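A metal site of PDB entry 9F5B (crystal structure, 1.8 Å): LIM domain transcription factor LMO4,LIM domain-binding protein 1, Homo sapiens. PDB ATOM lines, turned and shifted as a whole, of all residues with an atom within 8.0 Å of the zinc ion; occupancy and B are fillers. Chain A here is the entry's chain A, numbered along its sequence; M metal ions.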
ATOM      1  N   ALA A  71      -7.366   2.371  -7.046  1.00  0.00           N
ATOM      2  CA  ALA A  71      -8.650   2.249  -6.360  1.00  0.00           C
ATOM      3  C   ALA A  71      -9.431   1.090  -6.968  1.00  0.00           C
ATOM      4  O   ALA A  71      -9.366   0.844  -8.170  1.00  0.00           O
ATOM      5  CB  ALA A  71      -9.435   3.550  -6.483  1.00  0.00           C
ATOM      6  N   CYS A  72     -10.180   0.396  -6.103  1.00  0.00           N
ATOM      7  CA  CYS A  72     -10.940  -0.772  -6.508  1.00  0.00           C
ATOM      8  C   CYS A  72     -12.225  -0.358  -7.223  1.00  0.00           C
ATOM      9  O   CYS A  72     -13.000   0.443  -6.692  1.00  0.00           O
ATOM     10  CB  CYS A  72     -11.258  -1.619  -5.290  1.00  0.00           C
ATOM     11  SG  CYS A  72     -12.140  -3.121  -5.694  1.00  0.00           S
ATOM     12  N   SER A  73     -12.439  -0.882  -8.435  1.00  0.00           N
ATOM     13  CA  SER A  73     -13.648  -0.547  -9.198  1.00  0.00           C
ATOM     14  C   SER A  73     -14.918  -1.108  -8.568  1.00  0.00           C
ATOM     15  O   SER A  73     -15.999  -0.600  -8.825  1.00  0.00           O
ATOM     16  CB  SER A  73     -13.550  -1.059 -10.630  1.00  0.00           C
ATOM     17  OG  SER A  73     -12.743  -0.237 -11.429  1.00  0.00           O
ATOM     18  N   ALA A  74     -14.798  -2.149  -7.748  1.00  0.00           N
ATOM     19  CA  ALA A  74     -15.946  -2.766  -7.107  1.00  0.00           C
ATOM     20  C   ALA A  74     -16.381  -1.981  -5.874  1.00  0.00           C
ATOM     21  O   ALA A  74     -17.553  -1.629  -5.724  1.00  0.00           O
ATOM     22  CB  ALA A  74     -15.637  -4.216  -6.744  1.00  0.00           C
ATOM     23  N   CYS A  75     -15.450  -1.766  -4.926  1.00  0.00           N
ATOM     24  CA  CYS A  75     -15.806  -1.167  -3.650  1.00  0.00           C
ATOM     25  C   CYS A  75     -15.425   0.320  -3.549  1.00  0.00           C
ATOM     26  O   CYS A  75     -15.803   0.976  -2.567  1.00  0.00           O
ATOM     27  CB  CYS A  75     -15.196  -1.932  -2.475  1.00  0.00           C
ATOM     28  SG  CYS A  75     -13.412  -1.718  -2.364  1.00  0.00           S
ATOM     29  N   GLY A  76     -14.672   0.846  -4.507  1.00  0.00           N
ATOM     30  CA  GLY A  76     -14.342   2.264  -4.494  1.00  0.00           C
ATOM     31  C   GLY A  76     -13.183   2.685  -3.593  1.00  0.00           C
ATOM     32  O   GLY A  76     -12.808   3.864  -3.623  1.00  0.00           O
ATOM     33  N   GLN A  77     -12.612   1.770  -2.805  1.00  0.00           N
ATOM     34  CA  GLN A  77     -11.584   2.135  -1.847  1.00  0.00           C
ATOM     35  C   GLN A  77     -10.185   2.085  -2.475  1.00  0.00           C
ATOM     36  O   GLN A  77      -9.916   1.279  -3.362  1.00  0.00           O
ATOM     37  CB  GLN A  77     -11.624   1.240  -0.609  1.00  0.00           C
ATOM     38  CG  GLN A  77     -12.988   1.161   0.060  1.00  0.00           C
ATOM     39  CD  GLN A  77     -13.600   2.516   0.346  1.00  0.00           C
ATOM     40  OE1 GLN A  77     -13.292   3.179   1.347  1.00  0.00           O
ATOM     41  NE2 GLN A  77     -14.507   2.951  -0.536  1.00  0.00           N
ATOM     42  N   SER A  78      -9.315   2.987  -2.022  1.00  0.00           N
ATOM     43  CA  SER A  78      -7.917   3.043  -2.456  1.00  0.00           C
ATOM     44  C   SER A  78      -7.226   1.681  -2.302  1.00  0.00           C
ATOM     45  O   SER A  78      -7.602   0.854  -1.475  1.00  0.00           O
ATOM     46  CB  SER A  78      -7.169   4.144  -1.720  1.00  0.00           C
ATOM     47  OG  SER A  78      -7.244   3.939  -0.317  1.00  0.00           O
ATOM     48  N   ILE A  79      -6.237   1.442  -3.176  1.00  0.00           N
ATOM     49  CA  ILE A  79      -5.408   0.252  -3.126  1.00  0.00           C
ATOM     50  C   ILE A  79      -3.945   0.681  -3.010  1.00  0.00           C
ATOM     51  O   ILE A  79      -3.477   1.442  -3.853  1.00  0.00           O
ATOM     52  CB  ILE A  79      -5.600  -0.656  -4.355  1.00  0.00           C
ATOM     53  CG1 ILE A  79      -7.067  -1.074  -4.523  1.00  0.00           C
ATOM     54  CG2 ILE A  79      -4.693  -1.872  -4.246  1.00  0.00           C
ATOM     55  CD1 ILE A  79      -7.329  -1.795  -5.845  1.00  0.00           C
ATOM     56  N   GLU A  83      -0.021  -3.649  -2.866  1.00  0.00           N
ATOM     57  CA  GLU A  83      -1.024  -4.704  -2.818  1.00  0.00           C
ATOM     58  C   GLU A  83      -1.201  -5.368  -4.174  1.00  0.00           C
ATOM     59  O   GLU A  83      -1.173  -4.714  -5.215  1.00  0.00           O
ATOM     60  CB  GLU A  83      -2.356  -4.144  -2.335  1.00  0.00           C
ATOM     61  CG  GLU A  83      -3.384  -5.241  -2.138  1.00  0.00           C
ATOM     62  CD  GLU A  83      -4.637  -4.742  -1.458  1.00  0.00           C
ATOM     63  OE1 GLU A  83      -4.577  -3.730  -0.716  1.00  0.00           O
ATOM     64  OE2 GLU A  83      -5.678  -5.386  -1.676  1.00  0.00           O
ATOM     65  N   VAL A  92      -9.077  -2.241 -11.799  1.00  0.00           N
ATOM     66  CA  VAL A  92      -8.372  -3.038 -10.814  1.00  0.00           C
ATOM     67  C   VAL A  92      -9.312  -3.325  -9.646  1.00  0.00           C
ATOM     68  O   VAL A  92     -10.224  -2.553  -9.359  1.00  0.00           O
ATOM     69  CB  VAL A  92      -7.076  -2.378 -10.314  1.00  0.00           C
ATOM     70  CG1 VAL A  92      -6.090  -2.243 -11.473  1.00  0.00           C
ATOM     71  CG2 VAL A  92      -7.373  -1.042  -9.667  1.00  0.00           C
ATOM     72  N   TYR A  93      -9.073  -4.453  -8.991  1.00  0.00           N
ATOM     73  CA  TYR A  93      -9.952  -4.898  -7.925  1.00  0.00           C
ATOM     74  C   TYR A  93      -9.119  -5.459  -6.785  1.00  0.00           C
ATOM     75  O   TYR A  93      -8.102  -6.111  -7.022  1.00  0.00           O
ATOM     76  CB  TYR A  93     -10.893  -5.996  -8.435  1.00  0.00           C
ATOM     77  CG  TYR A  93     -11.789  -5.581  -9.563  1.00  0.00           C
ATOM     78  CD1 TYR A  93     -11.365  -5.704 -10.875  1.00  0.00           C
ATOM     79  CD2 TYR A  93     -13.051  -5.054  -9.316  1.00  0.00           C
ATOM     80  CE1 TYR A  93     -12.187  -5.333 -11.919  1.00  0.00           C
ATOM     81  CE2 TYR A  93     -13.880  -4.694 -10.358  1.00  0.00           C
ATOM     82  CZ  TYR A  93     -13.447  -4.822 -11.661  1.00  0.00           C
ATOM     83  OH  TYR A  93     -14.260  -4.447 -12.702  1.00  0.00           O
ATOM     84  N   HIS A  94      -9.562  -5.206  -5.548  1.00  0.00           N
ATOM     85  CA  HIS A  94      -9.104  -6.033  -4.423  1.00  0.00           C
ATOM     86  C   HIS A  94      -9.366  -7.491  -4.768  1.00  0.00           C
ATOM     87  O   HIS A  94     -10.385  -7.828  -5.401  1.00  0.00           O
ATOM     88  CB  HIS A  94      -9.855  -5.672  -3.140  1.00  0.00           C
ATOM     89  CG  HIS A  94      -9.565  -4.295  -2.622  1.00  0.00           C
ATOM     90  ND1 HIS A  94     -10.513  -3.289  -2.604  1.00  0.00           N
ATOM     91  CD2 HIS A  94      -8.451  -3.768  -2.063  1.00  0.00           C
ATOM     92  CE1 HIS A  94      -9.976  -2.201  -2.065  1.00  0.00           C
ATOM     93  NE2 HIS A  94      -8.735  -2.458  -1.740  1.00  0.00           N
ATOM     94  N   LEU A  95      -8.455  -8.378  -4.333  1.00  0.00           N
ATOM     95  CA  LEU A  95      -8.651  -9.801  -4.570  1.00  0.00           C
ATOM     96  C   LEU A  95     -10.023 -10.255  -4.072  1.00  0.00           C
ATOM     97  O   LEU A  95     -10.719 -11.005  -4.743  1.00  0.00           O
ATOM     98  CB  LEU A  95      -7.533 -10.622  -3.949  1.00  0.00           C
ATOM     99  CG  LEU A  95      -6.394 -10.957  -4.918  1.00  0.00           C
ATOM    100  CD1 LEU A  95      -5.735  -9.696  -5.460  1.00  0.00           C
ATOM    101  CD2 LEU A  95      -5.381 -11.905  -4.341  1.00  0.00           C
ATOM    102  N   LYS A  96     -10.424  -9.823  -2.884  1.00  0.00           N
ATOM    103  CA  LYS A  96     -11.690 -10.305  -2.334  1.00  0.00           C
ATOM    104  C   LYS A  96     -12.892  -9.600  -2.950  1.00  0.00           C
ATOM    105  O   LYS A  96     -14.017 -10.042  -2.733  1.00  0.00           O
ATOM    106  CB  LYS A  96     -11.770 -10.337  -0.813  1.00  0.00           C
ATOM    107  CG  LYS A  96     -10.923 -11.480  -0.263  1.00  0.00           C
ATOM    108  CD  LYS A  96     -10.980 -11.749   1.238  1.00  0.00           C
ATOM    109  CE  LYS A  96      -9.992 -12.829   1.622  1.00  0.00           C
ATOM    110  NZ  LYS A  96      -9.986 -13.322   2.997  1.00  0.00           N
ATOM    111  N   CYS A  97     -12.662  -8.555  -3.720  1.00  0.00           N
ATOM    112  CA  CYS A  97     -13.740  -7.902  -4.438  1.00  0.00           C
ATOM    113  C   CYS A  97     -13.955  -8.486  -5.833  1.00  0.00           C
ATOM    114  O   CYS A  97     -14.931  -8.119  -6.494  1.00  0.00           O
ATOM    115  CB  CYS A  97     -13.451  -6.414  -4.528  1.00  0.00           C
ATOM    116  SG  CYS A  97     -13.591  -5.628  -2.905  1.00  0.00           S
ATOM    117  N   PHE A  98     -13.082  -9.384  -6.286  1.00  0.00           N
ATOM    118  CA  PHE A  98     -13.149  -9.923  -7.636  1.00  0.00           C
ATOM    119  C   PHE A  98     -14.069 -11.139  -7.630  1.00  0.00           C
ATOM    120  O   PHE A  98     -13.611 -12.282  -7.679  1.00  0.00           O
ATOM    121  CB  PHE A  98     -11.726 -10.216  -8.123  1.00  0.00           C
ATOM    122  CG  PHE A  98     -11.583 -10.329  -9.627  1.00  0.00           C
ATOM    123  CD1 PHE A  98     -11.787  -9.209 -10.433  1.00  0.00           C
ATOM    124  CD2 PHE A  98     -11.215 -11.522 -10.223  1.00  0.00           C
ATOM    125  CE1 PHE A  98     -11.639  -9.301 -11.807  1.00  0.00           C
ATOM    126  CE2 PHE A  98     -11.053 -11.623 -11.595  1.00  0.00           C
ATOM    127  CZ  PHE A  98     -11.261 -10.499 -12.394  1.00  0.00           C
HETATM  128 ZN    ZN M   1     -12.600  -3.653  -3.375  1.00  0.00          ZN
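The zinc ion is bound by a ring nitrogen (ND1) of His 94, the side-chain sulfur of Cys 97, the side-chain sulfur of Cys 75 and the side-chain sulfur of Cys 72.
The zinc ion has four donor atoms within binding distance.
Four residues have an atom within 4 Å of the zinc ion: Cys 72, Cys 75, His 94 and Cys 97.
The nearest printed residue that does not touch the zinc ion is Ala 74 (4.6 Å).
The backbone carbonyl oxygen of Cys 75 lies within hydrogen-bond range of the side-chain amide nitrogen of Gln 77 (3.1 Å).
SG of Cys 72 lies close to N of Ala 74.
The backbone NH of Cys 72 lies within hydrogen-bond range of the backbone carbonyl oxygen of Gln 77, 2.9 Å away.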
